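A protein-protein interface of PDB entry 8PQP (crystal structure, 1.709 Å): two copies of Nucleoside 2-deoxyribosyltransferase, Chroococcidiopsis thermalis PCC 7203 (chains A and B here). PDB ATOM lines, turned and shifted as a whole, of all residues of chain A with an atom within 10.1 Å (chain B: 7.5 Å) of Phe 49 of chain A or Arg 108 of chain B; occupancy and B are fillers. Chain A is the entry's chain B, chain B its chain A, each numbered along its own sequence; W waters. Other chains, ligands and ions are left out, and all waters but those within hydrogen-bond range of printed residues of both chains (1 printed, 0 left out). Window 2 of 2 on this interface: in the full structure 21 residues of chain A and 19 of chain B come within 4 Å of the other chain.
Of the printed residues of chain B, Asp 48 of chain A touches Phe 106 (3.5 Å). Phe 49 of chain A touches three residues of chain B. Thr 79 of chain B touches none of the printed residues of chain A. Of the printed residues of chain A, Asp 105 of chain B touches Phe 14. Arg 108 of chain B touches just one residue of chain A: Phe 49 (3.3 Å). Ser 110 of chain B touches none of the printed residues of chain A. No residue of chain A comes within 4 Å of Pro 116 of chain B. The nearest residue of chain A that does not touch Arg 108 of chain B is Phe 14 of chain A (7.9 Å). The nearest printed residue of chain A that does not touch Asp 105 of chain B is Ser 15 of chain A (4.1 Å).
Water W1 bridges OE1 of Glu 83 of chain A (2.9 Å) and NH1 of Arg 107 of chain B (3.1 Å).
No position is printed for both chains. Of the 8 pairs that touch across the chains among the printed residues, none has its exchanged pair printed and touching as well.
N of Phe 106 of chain B lies within hydrogen-bond range of O of Phe 14 of chain A (2.9 Å).
Printed residues of chain B that touch a printed residue of chain A: Asp 105, Phe 106, Arg 107 and Arg 108. Hydrophobic or aromatic side chains of chain B within 4 Å of the printed part of chain A: Phe 106. Of the 18 printed residues of chain A, 4 touch a printed residue of chain B. Among the printed residues, 8 pairs touch across the chains.
The side-chain carboxylate (OD2) of Asp 105 of chain B lies within salt-bridge range of the guanidinium group (NH2) of Arg 107 of chain B. The guanidinium group (NH2) of Arg 103 of chain B is in salt-bridge range of the side-chain carboxylate (OD2) of Asp 105 of chain B (3.2 Å). The backbone carbonyl oxygen (O) of Arg 107 of chain B sits at hydrogen-bond distance from the guanidinium group (NH2) of Arg 103 of chain B (3.0 Å).
Among the printed residues, merely in contact across the chains: Phe 49 of chain A with Phe 106 of chain B (3.0 Å), Phe 14 of chain A with Asp 105 of chain B (3.3 Å), Phe 49 of chain A with Arg 108 of chain B (3.3 Å), Gly 13 of chain A with Phe 106 of chain B (3.5 Å), Asp 48 of chain A with Phe 106 of chain B (3.5 Å), Phe 14 of chain A with Arg 107 of chain B (3.6 Å) and Phe 49 of chain A with Arg 107 of chain B (3.8 Å).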
ATOM      1  N   GLY A  13     -39.989 -19.472  16.522  1.00  0.00           N
ATOM      2  CA  GLY A  13     -39.175 -19.064  17.652  1.00  0.00           C
ATOM      3  C   GLY A  13     -37.765 -18.628  17.292  1.00  0.00           C
ATOM      4  O   GLY A  13     -37.071 -18.084  18.156  1.00  0.00           O
ATOM      5  N   PHE A  14     -37.324 -18.858  16.052  1.00  0.00           N
ATOM      6  CA  PHE A  14     -35.979 -18.476  15.641  1.00  0.00           C
ATOM      7  C   PHE A  14     -35.862 -16.988  15.326  1.00  0.00           C
ATOM      8  O   PHE A  14     -34.761 -16.431  15.417  1.00  0.00           O
ATOM      9  CB  PHE A  14     -35.553 -19.289  14.410  1.00  0.00           C
ATOM     10  CG  PHE A  14     -35.367 -20.757  14.683  1.00  0.00           C
ATOM     11  CD1 PHE A  14     -34.553 -21.187  15.714  1.00  0.00           C
ATOM     12  CD2 PHE A  14     -36.007 -21.707  13.894  1.00  0.00           C
ATOM     13  CE1 PHE A  14     -34.386 -22.538  15.973  1.00  0.00           C
ATOM     14  CE2 PHE A  14     -35.842 -23.055  14.139  1.00  0.00           C
ATOM     15  CZ  PHE A  14     -35.030 -23.472  15.183  1.00  0.00           C
ATOM     16  N   SER A  15     -36.958 -16.331  14.961  1.00  0.00           N
ATOM     17  CA  SER A  15     -36.950 -14.903  14.669  1.00  0.00           C
ATOM     18  C   SER A  15     -37.665 -14.144  15.779  1.00  0.00           C
ATOM     19  O   SER A  15     -38.744 -14.550  16.225  1.00  0.00           O
ATOM     20  CB  SER A  15     -37.613 -14.626  13.318  1.00  0.00           C
ATOM     21  OG  SER A  15     -38.170 -13.327  13.262  1.00  0.00           O
ATOM     22  N   LYS A  19     -41.411 -14.772  16.613  1.00  0.00           N
ATOM     23  CA  LYS A  19     -41.714 -15.321  17.938  1.00  0.00           C
ATOM     24  C   LYS A  19     -42.749 -14.478  18.674  1.00  0.00           C
ATOM     25  O   LYS A  19     -43.686 -15.012  19.283  1.00  0.00           O
ATOM     26  CB  LYS A  19     -40.430 -15.422  18.761  1.00  0.00           C
ATOM     27  CG  LYS A  19     -40.635 -15.896  20.191  1.00  0.00           C
ATOM     28  CD  LYS A  19     -39.300 -16.056  20.900  1.00  0.00           C
ATOM     29  CE  LYS A  19     -39.500 -16.408  22.369  1.00  0.00           C
ATOM     30  NZ  LYS A  19     -39.032 -17.787  22.673  1.00  0.00           N
ATOM     31  N   PHE A  41     -40.670 -23.693  22.052  1.00  0.00           N
ATOM     32  CA  PHE A  41     -39.690 -22.632  22.263  1.00  0.00           C
ATOM     33  C   PHE A  41     -39.807 -22.059  23.672  1.00  0.00           C
ATOM     34  O   PHE A  41     -38.798 -21.895  24.366  1.00  0.00           O
ATOM     35  CB  PHE A  41     -39.842 -21.552  21.188  1.00  0.00           C
ATOM     36  CG  PHE A  41     -39.243 -21.941  19.852  1.00  0.00           C
ATOM     37  CD1 PHE A  41     -37.868 -21.972  19.676  1.00  0.00           C
ATOM     38  CD2 PHE A  41     -40.058 -22.288  18.779  1.00  0.00           C
ATOM     39  CE1 PHE A  41     -37.313 -22.335  18.452  1.00  0.00           C
ATOM     40  CE2 PHE A  41     -39.515 -22.653  17.560  1.00  0.00           C
ATOM     41  CZ  PHE A  41     -38.136 -22.675  17.395  1.00  0.00           C
ATOM     42  N   ASN A  45     -37.506 -23.558  26.948  1.00  0.00           N
ATOM     43  CA  ASN A  45     -36.668 -22.363  27.059  1.00  0.00           C
ATOM     44  C   ASN A  45     -35.540 -22.359  26.025  1.00  0.00           C
ATOM     45  O   ASN A  45     -34.352 -22.353  26.348  1.00  0.00           O
ATOM     46  CB  ASN A  45     -36.123 -22.205  28.478  1.00  0.00           C
ATOM     47  CG  ASN A  45     -36.249 -20.779  28.986  1.00  0.00           C
ATOM     48  OD1 ASN A  45     -35.520 -19.884  28.552  1.00  0.00           O
ATOM     49  ND2 ASN A  45     -37.193 -20.556  29.894  1.00  0.00           N
ATOM     50  N   GLN A  46     -35.944 -22.356  24.757  1.00  0.00           N
ATOM     51  CA  GLN A  46     -35.029 -22.256  23.622  1.00  0.00           C
ATOM     52  C   GLN A  46     -35.182 -20.852  23.039  1.00  0.00           C
ATOM     53  O   GLN A  46     -35.854 -20.642  22.028  1.00  0.00           O
ATOM     54  CB  GLN A  46     -35.327 -23.355  22.583  1.00  0.00           C
ATOM     55  CG  GLN A  46     -34.363 -23.369  21.397  1.00  0.00           C
ATOM     56  CD  GLN A  46     -34.630 -24.497  20.406  1.00  0.00           C
ATOM     57  OE1 GLN A  46     -35.646 -25.194  20.486  1.00  0.00           O
ATOM     58  NE2 GLN A  46     -33.712 -24.677  19.461  1.00  0.00           N
ATOM     59  N   ILE A  47     -34.547 -19.880  23.696  1.00  0.00           N
ATOM     60  CA  ILE A  47     -34.773 -18.466  23.410  1.00  0.00           C
ATOM     61  C   ILE A  47     -33.599 -17.795  22.703  1.00  0.00           C
ATOM     62  O   ILE A  47     -33.761 -16.668  22.202  1.00  0.00           O
ATOM     63  CB  ILE A  47     -35.138 -17.686  24.693  1.00  0.00           C
ATOM     64  CG1 ILE A  47     -33.978 -17.698  25.690  1.00  0.00           C
ATOM     65  CG2 ILE A  47     -36.379 -18.284  25.342  1.00  0.00           C
ATOM     66  CD1 ILE A  47     -34.254 -16.886  26.942  1.00  0.00           C
ATOM     67  N   ASP A  48     -32.436 -18.436  22.640  1.00  0.00           N
ATOM     68  CA  ASP A  48     -31.295 -17.931  21.887  1.00  0.00           C
ATOM     69  C   ASP A  48     -30.508 -19.132  21.377  1.00  0.00           C
ATOM     70  O   ASP A  48     -30.983 -20.271  21.417  1.00  0.00           O
ATOM     71  CB  ASP A  48     -30.442 -16.990  22.750  1.00  0.00           C
ATOM     72  N   PHE A  49     -29.298 -18.876  20.887  1.00  0.00           N
ATOM     73  CA  PHE A  49     -28.398 -19.959  20.514  1.00  0.00           C
ATOM     74  C   PHE A  49     -28.011 -20.760  21.756  1.00  0.00           C
ATOM     75  O   PHE A  49     -27.782 -20.195  22.832  1.00  0.00           O
ATOM     76  CB  PHE A  49     -27.155 -19.393  19.824  1.00  0.00           C
ATOM     77  CG  PHE A  49     -26.803 -20.080  18.536  1.00  0.00           C
ATOM     78  CD1 PHE A  49     -27.452 -19.767  17.356  1.00  0.00           C
ATOM     79  CD2 PHE A  49     -25.820 -21.051  18.508  1.00  0.00           C
ATOM     80  CE1 PHE A  49     -27.114 -20.414  16.175  1.00  0.00           C
ATOM     81  CE2 PHE A  49     -25.491 -21.692  17.334  1.00  0.00           C
ATOM     82  CZ  PHE A  49     -26.135 -21.375  16.168  1.00  0.00           C
ATOM     83  N   SER A  50     -27.930 -22.084  21.607  1.00  0.00           N
ATOM     84  CA  SER A  50     -27.802 -23.002  22.739  1.00  0.00           C
ATOM     85  C   SER A  50     -26.368 -23.502  22.926  1.00  0.00           C
ATOM     86  O   SER A  50     -25.658 -23.769  21.953  1.00  0.00           O
ATOM     87  CB  SER A  50     -28.746 -24.198  22.578  1.00  0.00           C
ATOM     88  OG  SER A  50     -28.630 -25.080  23.691  1.00  0.00           O
ATOM     89  N   GLN A  51     -25.972 -23.690  24.187  1.00  0.00           N
ATOM     90  CA  GLN A  51     -24.572 -23.859  24.545  1.00  0.00           C
ATOM     91  C   GLN A  51     -24.146 -25.321  24.438  1.00  0.00           C
ATOM     92  O   GLN A  51     -24.850 -26.165  23.881  1.00  0.00           O
ATOM     93  CB  GLN A  51     -24.321 -23.375  25.967  1.00  0.00           C
ATOM     94  CG  GLN A  51     -24.462 -21.869  26.252  1.00  0.00           C
ATOM     95  CD  GLN A  51     -24.633 -21.604  27.740  1.00  0.00           C
ATOM     96  OE1 GLN A  51     -25.384 -22.309  28.415  1.00  0.00           O
ATOM     97  NE2 GLN A  51     -23.915 -20.615  28.263  1.00  0.00           N
ATOM     98  N   ALA A  52     -22.971 -25.619  24.998  1.00  0.00           N
ATOM     99  CA  ALA A  52     -22.252 -26.874  24.851  1.00  0.00           C
ATOM    100  C   ALA A  52     -22.686 -27.930  25.841  1.00  0.00           C
ATOM    101  O   ALA A  52     -22.088 -29.009  25.848  1.00  0.00           O
ATOM    102  CB  ALA A  52     -20.732 -26.660  25.013  1.00  0.00           C
ATOM    103  N   ASP A  53     -23.610 -27.613  26.742  1.00  0.00           N
ATOM    104  CA  ASP A  53     -24.080 -28.557  27.749  1.00  0.00           C
ATOM    105  C   ASP A  53     -25.591 -28.690  27.725  1.00  0.00           C
ATOM    106  O   ASP A  53     -26.166 -29.409  28.554  1.00  0.00           O
ATOM    107  CB  ASP A  53     -23.616 -28.143  29.167  1.00  0.00           C
ATOM    108  CG  ASP A  53     -23.784 -26.640  29.432  1.00  0.00           C
ATOM    109  OD1 ASP A  53     -23.858 -25.873  28.432  1.00  0.00           O
ATOM    110  OD2 ASP A  53     -23.792 -26.199  30.602  1.00  0.00           O
ATOM    111  N   TRP A  54     -26.248 -28.015  26.798  1.00  0.00           N
ATOM    112  CA  TRP A  54     -27.676 -27.771  26.880  1.00  0.00           C
ATOM    113  C   TRP A  54     -28.462 -28.229  25.662  1.00  0.00           C
ATOM    114  O   TRP A  54     -29.672 -28.436  25.777  1.00  0.00           O
ATOM    115  CB  TRP A  54     -27.947 -26.268  27.064  1.00  0.00           C
ATOM    116  CG  TRP A  54     -28.215 -25.728  28.459  1.00  0.00           C
ATOM    117  CD1 TRP A  54     -27.480 -24.782  29.122  1.00  0.00           C
ATOM    118  CD2 TRP A  54     -29.343 -26.022  29.309  1.00  0.00           C
ATOM    119  NE1 TRP A  54     -28.059 -24.494  30.337  1.00  0.00           N
ATOM    120  CE2 TRP A  54     -29.201 -25.241  30.477  1.00  0.00           C
ATOM    121  CE3 TRP A  54     -30.445 -26.883  29.203  1.00  0.00           C
ATOM    122  CZ2 TRP A  54     -30.121 -25.293  31.532  1.00  0.00           C
ATOM    123  CZ3 TRP A  54     -31.362 -26.932  30.257  1.00  0.00           C
ATOM    124  CH2 TRP A  54     -31.190 -26.142  31.404  1.00  0.00           C
ATOM    125  N   ALA A  55     -27.831 -28.354  24.499  1.00  0.00           N
ATOM    126  CA  ALA A  55     -28.588 -28.637  23.290  1.00  0.00           C
ATOM    127  C   ALA A  55     -29.053 -30.089  23.225  1.00  0.00           C
ATOM    128  O   ALA A  55     -30.090 -30.370  22.617  1.00  0.00           O
ATOM    129  CB  ALA A  55     -27.760 -28.267  22.060  1.00  0.00           C
ATOM    130  N   VAL A  58     -32.310 -30.157  25.224  1.00  0.00           N
ATOM    131  CA  VAL A  58     -33.405 -29.584  24.443  1.00  0.00           C
ATOM    132  C   VAL A  58     -33.948 -30.618  23.464  1.00  0.00           C
ATOM    133  O   VAL A  58     -35.162 -30.825  23.360  1.00  0.00           O
ATOM    134  CB  VAL A  58     -32.944 -28.301  23.722  1.00  0.00           C
ATOM    135  CG1 VAL A  58     -34.015 -27.797  22.733  1.00  0.00           C
ATOM    136  CG2 VAL A  58     -32.586 -27.220  24.728  1.00  0.00           C
ATOM    137  N   GLU A  83     -36.400 -27.864   9.239  1.00  0.00           N
ATOM    138  CA  GLU A  83     -35.898 -29.229   9.372  1.00  0.00           C
ATOM    139  C   GLU A  83     -36.255 -29.837  10.716  1.00  0.00           C
ATOM    140  O   GLU A  83     -36.459 -31.051  10.793  1.00  0.00           O
ATOM    141  CB  GLU A  83     -34.386 -29.285   9.169  1.00  0.00           C
ATOM    142  CG  GLU A  83     -33.579 -28.439  10.137  1.00  0.00           C
ATOM    143  CD  GLU A  83     -33.228 -27.105   9.545  1.00  0.00           C
ATOM    144  OE1 GLU A  83     -32.175 -26.541   9.906  1.00  0.00           O
ATOM    145  OE2 GLU A  83     -34.025 -26.615   8.722  1.00  0.00           O
ATOM    146  N   THR B  79     -33.286 -19.853   6.464  1.00  0.00           N
ATOM    147  CA  THR B  79     -32.136 -20.655   6.057  1.00  0.00           C
ATOM    148  C   THR B  79     -32.580 -21.442   4.830  1.00  0.00           C
ATOM    149  O   THR B  79     -33.282 -22.458   4.954  1.00  0.00           O
ATOM    150  CB  THR B  79     -31.641 -21.572   7.176  1.00  0.00           C
ATOM    151  OG1 THR B  79     -32.695 -22.447   7.599  1.00  0.00           O
ATOM    152  CG2 THR B  79     -31.150 -20.742   8.373  1.00  0.00           C
ATOM    153  N   ARG B 103     -31.887  -9.053   9.647  1.00  0.00           N
ATOM    154  CA  ARG B 103     -32.005 -10.457  10.059  1.00  0.00           C
ATOM    155  C   ARG B 103     -32.164 -10.516  11.573  1.00  0.00           C
ATOM    156  O   ARG B 103     -31.218 -10.227  12.313  1.00  0.00           O
ATOM    157  CB  ARG B 103     -30.790 -11.270   9.598  1.00  0.00           C
ATOM    158  CG  ARG B 103     -30.723 -12.693  10.201  1.00  0.00           C
ATOM    159  CD  ARG B 103     -29.734 -13.612   9.440  1.00  0.00           C
ATOM    160  NE  ARG B 103     -29.772 -14.987   9.952  1.00  0.00           N
ATOM    161  CZ  ARG B 103     -30.392 -15.999   9.354  1.00  0.00           C
ATOM    162  NH1 ARG B 103     -31.017 -15.807   8.195  1.00  0.00           N
ATOM    163  NH2 ARG B 103     -30.387 -17.203   9.920  1.00  0.00           N
ATOM    164  N   ASP B 105     -33.269 -13.456  12.860  1.00  0.00           N
ATOM    165  CA  ASP B 105     -33.188 -14.908  12.995  1.00  0.00           C
ATOM    166  C   ASP B 105     -31.892 -15.242  13.725  1.00  0.00           C
ATOM    167  O   ASP B 105     -30.816 -14.829  13.282  1.00  0.00           O
ATOM    168  CB  ASP B 105     -33.225 -15.496  11.577  1.00  0.00           C
ATOM    169  CG  ASP B 105     -33.267 -17.024  11.523  1.00  0.00           C
ATOM    170  OD1 ASP B 105     -33.007 -17.711  12.532  1.00  0.00           O
ATOM    171  OD2 ASP B 105     -33.542 -17.535  10.408  1.00  0.00           O
ATOM    172  N   PHE B 106     -31.971 -15.960  14.845  1.00  0.00           N
ATOM    173  CA  PHE B 106     -30.757 -16.212  15.618  1.00  0.00           C
ATOM    174  C   PHE B 106     -29.961 -17.414  15.125  1.00  0.00           C
ATOM    175  O   PHE B 106     -28.893 -17.699  15.679  1.00  0.00           O
ATOM    176  CB  PHE B 106     -31.066 -16.333  17.134  1.00  0.00           C
ATOM    177  CG  PHE B 106     -31.761 -17.610  17.579  1.00  0.00           C
ATOM    178  CD1 PHE B 106     -31.114 -18.839  17.568  1.00  0.00           C
ATOM    179  CD2 PHE B 106     -33.041 -17.549  18.119  1.00  0.00           C
ATOM    180  CE1 PHE B 106     -31.754 -19.995  18.018  1.00  0.00           C
ATOM    181  CE2 PHE B 106     -33.687 -18.702  18.581  1.00  0.00           C
ATOM    182  CZ  PHE B 106     -33.042 -19.925  18.523  1.00  0.00           C
ATOM    183  N   ARG B 107     -30.429 -18.118  14.102  1.00  0.00           N
ATOM    184  CA  ARG B 107     -29.678 -19.266  13.615  1.00  0.00           C
ATOM    185  C   ARG B 107     -28.455 -18.795  12.839  1.00  0.00           C
ATOM    186  O   ARG B 107     -28.490 -17.766  12.157  1.00  0.00           O
ATOM    187  CB  ARG B 107     -30.554 -20.161  12.743  1.00  0.00           C
ATOM    188  CG  ARG B 107     -31.534 -20.985  13.536  1.00  0.00           C
ATOM    189  CD  ARG B 107     -32.550 -21.621  12.638  1.00  0.00           C
ATOM    190  NE  ARG B 107     -33.233 -20.611  11.847  1.00  0.00           N
ATOM    191  CZ  ARG B 107     -34.148 -20.889  10.930  1.00  0.00           C
ATOM    192  NH1 ARG B 107     -34.487 -22.155  10.683  1.00  0.00           N
ATOM    193  NH2 ARG B 107     -34.724 -19.904  10.258  1.00  0.00           N
ATOM    194  N   ARG B 108     -27.366 -19.551  12.968  1.00  0.00           N
ATOM    195  CA  ARG B 108     -26.077 -19.222  12.365  1.00  0.00           C
ATOM    196  C   ARG B 108     -25.899 -20.095  11.130  1.00  0.00           C
ATOM    197  O   ARG B 108     -25.753 -21.315  11.250  1.00  0.00           O
ATOM    198  CB  ARG B 108     -24.946 -19.454  13.369  1.00  0.00           C
ATOM    199  CG  ARG B 108     -23.573 -18.889  12.973  1.00  0.00           C
ATOM    200  CD  ARG B 108     -23.666 -17.727  11.986  1.00  0.00           C
ATOM    201  NE  ARG B 108     -24.244 -16.549  12.625  1.00  0.00           N
ATOM    202  CZ  ARG B 108     -23.573 -15.712  13.409  1.00  0.00           C
ATOM    203  NH1 ARG B 108     -24.193 -14.674  13.953  1.00  0.00           N
ATOM    204  NH2 ARG B 108     -22.284 -15.911  13.652  1.00  0.00           N
ATOM    205  N   CYS B 109     -25.908 -19.479   9.945  1.00  0.00           N
ATOM    206  CA  CYS B 109     -25.830 -20.226   8.681  1.00  0.00           C
ATOM    207  C   CYS B 109     -24.956 -19.451   7.693  1.00  0.00           C
ATOM    208  O   CYS B 109     -25.459 -18.649   6.901  1.00  0.00           O
ATOM    209  CB  CYS B 109     -27.212 -20.484   8.109  1.00  0.00           C
ATOM    210  SG  CYS B 109     -27.225 -21.835   6.912  1.00  0.00           S
ATOM    211  N   SER B 110     -23.655 -19.725   7.718  1.00  0.00           N
ATOM    212  CA  SER B 110     -22.698 -18.938   6.943  1.00  0.00           C
ATOM    213  C   SER B 110     -21.657 -19.855   6.317  1.00  0.00           C
ATOM    214  O   SER B 110     -21.576 -21.047   6.628  1.00  0.00           O
ATOM    215  CB  SER B 110     -22.011 -17.877   7.816  1.00  0.00           C
ATOM    216  OG  SER B 110     -20.908 -17.287   7.141  1.00  0.00           O
ATOM    217  N   ASP B 111     -20.852 -19.280   5.411  1.00  0.00           N
ATOM    218  CA  ASP B 111     -19.723 -19.990   4.816  1.00  0.00           C
ATOM    219  C   ASP B 111     -18.381 -19.359   5.185  1.00  0.00           C
ATOM    220  O   ASP B 111     -17.377 -19.617   4.515  1.00  0.00           O
ATOM    221  CB  ASP B 111     -19.871 -20.077   3.290  1.00  0.00           C
ATOM    222  CG  ASP B 111     -19.980 -18.715   2.625  1.00  0.00           C
ATOM    223  OD1 ASP B 111     -19.852 -17.678   3.309  1.00  0.00           O
ATOM    224  OD2 ASP B 111     -20.217 -18.679   1.403  1.00  0.00           O
ATOM    225  N   ASN B 112     -18.345 -18.537   6.236  1.00  0.00           N
ATOM    226  CA  ASN B 112     -17.139 -17.815   6.615  1.00  0.00           C
ATOM    227  C   ASN B 112     -17.298 -17.341   8.052  1.00  0.00           C
ATOM    228  O   ASN B 112     -18.385 -17.406   8.627  1.00  0.00           O
ATOM    229  CB  ASN B 112     -16.884 -16.637   5.681  1.00  0.00           C
ATOM    230  CG  ASN B 112     -17.915 -15.552   5.838  1.00  0.00           C
ATOM    231  OD1 ASN B 112     -17.690 -14.576   6.549  1.00  0.00           O
ATOM    232  ND2 ASN B 112     -19.064 -15.716   5.180  1.00  0.00           N
ATOM    233  N   GLU B 113     -16.196 -16.850   8.623  1.00  0.00           N
ATOM    234  CA  GLU B 113     -16.160 -16.470  10.032  1.00  0.00           C
ATOM    235  C   GLU B 113     -16.360 -14.976  10.266  1.00  0.00           C
ATOM    236  O   GLU B 113     -16.651 -14.582  11.400  1.00  0.00           O
ATOM    237  CB  GLU B 113     -14.822 -16.891  10.656  1.00  0.00           C
ATOM    238  CG  GLU B 113     -13.643 -16.202   9.981  1.00  0.00           C
ATOM    239  CD  GLU B 113     -12.285 -16.833  10.275  1.00  0.00           C
ATOM    240  OE1 GLU B 113     -11.807 -16.722  11.425  1.00  0.00           O
ATOM    241  OE2 GLU B 113     -11.674 -17.397   9.339  1.00  0.00           O
ATOM    242  N   ARG B 114     -16.205 -14.132   9.240  1.00  0.00           N
ATOM    243  CA  ARG B 114     -16.423 -12.702   9.438  1.00  0.00           C
ATOM    244  C   ARG B 114     -17.907 -12.359   9.410  1.00  0.00           C
ATOM    245  O   ARG B 114     -18.415 -11.675  10.308  1.00  0.00           O
ATOM    246  CB  ARG B 114     -15.683 -11.885   8.377  1.00  0.00           C
ATOM    247  CG  ARG B 114     -16.123 -10.426   8.365  1.00  0.00           C
ATOM    248  CD  ARG B 114     -15.044  -9.543   7.773  1.00  0.00           C
ATOM    249  NE  ARG B 114     -13.801  -9.627   8.536  1.00  0.00           N
ATOM    250  CZ  ARG B 114     -12.702  -8.960   8.212  1.00  0.00           C
ATOM    251  NH1 ARG B 114     -12.719  -8.183   7.143  1.00  0.00           N
ATOM    252  NH2 ARG B 114     -11.600  -9.068   8.943  1.00  0.00           N
ATOM    253  N   TYR B 115     -18.619 -12.837   8.399  1.00  0.00           N
ATOM    254  CA  TYR B 115     -19.999 -12.421   8.217  1.00  0.00           C
ATOM    255  C   TYR B 115     -20.974 -13.475   8.726  1.00  0.00           C
ATOM    256  O   TYR B 115     -20.661 -14.667   8.725  1.00  0.00           O
ATOM    257  CB  TYR B 115     -20.285 -12.185   6.739  1.00  0.00           C
ATOM    258  CG  TYR B 115     -19.378 -11.150   6.073  1.00  0.00           C
ATOM    259  CD1 TYR B 115     -19.535  -9.799   6.326  1.00  0.00           C
ATOM    260  CD2 TYR B 115     -18.386 -11.548   5.188  1.00  0.00           C
ATOM    261  CE1 TYR B 115     -18.725  -8.847   5.704  1.00  0.00           C
ATOM    262  CE2 TYR B 115     -17.570 -10.607   4.568  1.00  0.00           C
ATOM    263  CZ  TYR B 115     -17.751  -9.259   4.848  1.00  0.00           C
ATOM    264  OH  TYR B 115     -16.957  -8.305   4.243  1.00  0.00           O
ATOM    265  N   PRO B 116     -22.189 -13.065   9.109  1.00  0.00           N
ATOM    266  CA  PRO B 116     -23.159 -14.031   9.651  1.00  0.00           C
ATOM    267  C   PRO B 116     -23.945 -14.796   8.604  1.00  0.00           C
ATOM    268  O   PRO B 116     -24.664 -15.739   8.972  1.00  0.00           O
ATOM    269  CB  PRO B 116     -24.086 -13.149  10.506  1.00  0.00           C
ATOM    270  CG  PRO B 116     -24.009 -11.797   9.853  1.00  0.00           C
ATOM    271  CD  PRO B 116     -22.592 -11.668   9.359  1.00  0.00           C
ATOM    272  N   LEU B 117     -23.840 -14.436   7.326  1.00  0.00           N
ATOM    273  CA  LEU B 117     -24.465 -15.173   6.233  1.00  0.00           C
ATOM    274  C   LEU B 117     -23.431 -15.382   5.130  1.00  0.00           C
ATOM    275  O   LEU B 117     -22.294 -14.914   5.225  1.00  0.00           O
ATOM    276  CB  LEU B 117     -25.686 -14.425   5.692  1.00  0.00           C
ATOM    277  CG  LEU B 117     -26.831 -14.214   6.674  1.00  0.00           C
ATOM    278  CD1 LEU B 117     -27.658 -13.036   6.239  1.00  0.00           C
ATOM    279  CD2 LEU B 117     -27.685 -15.474   6.754  1.00  0.00           C
ATOM    280  N   TYR B 134     -26.216  -3.638   9.135  1.00  0.00           N
ATOM    281  CA  TYR B 134     -26.773  -4.952   9.435  1.00  0.00           C
ATOM    282  C   TYR B 134     -27.635  -4.802  10.676  1.00  0.00           C
ATOM    283  O   TYR B 134     -27.119  -4.479  11.748  1.00  0.00           O
ATOM    284  CB  TYR B 134     -25.659  -5.982   9.658  1.00  0.00           C
ATOM    285  CG  TYR B 134     -26.128  -7.422   9.832  1.00  0.00           C
ATOM    286  CD1 TYR B 134     -26.455  -8.185   8.727  1.00  0.00           C
ATOM    287  CD2 TYR B 134     -26.218  -8.016  11.088  1.00  0.00           C
ATOM    288  CE1 TYR B 134     -26.883  -9.492   8.858  1.00  0.00           C
ATOM    289  CE2 TYR B 134     -26.650  -9.345  11.230  1.00  0.00           C
ATOM    290  CZ  TYR B 134     -26.973 -10.067  10.093  1.00  0.00           C
ATOM    291  OH  TYR B 134     -27.398 -11.375  10.183  1.00  0.00           O
HETATM  292  O   HOH W   1     -33.881 -25.003  11.651  1.00  0.00           O
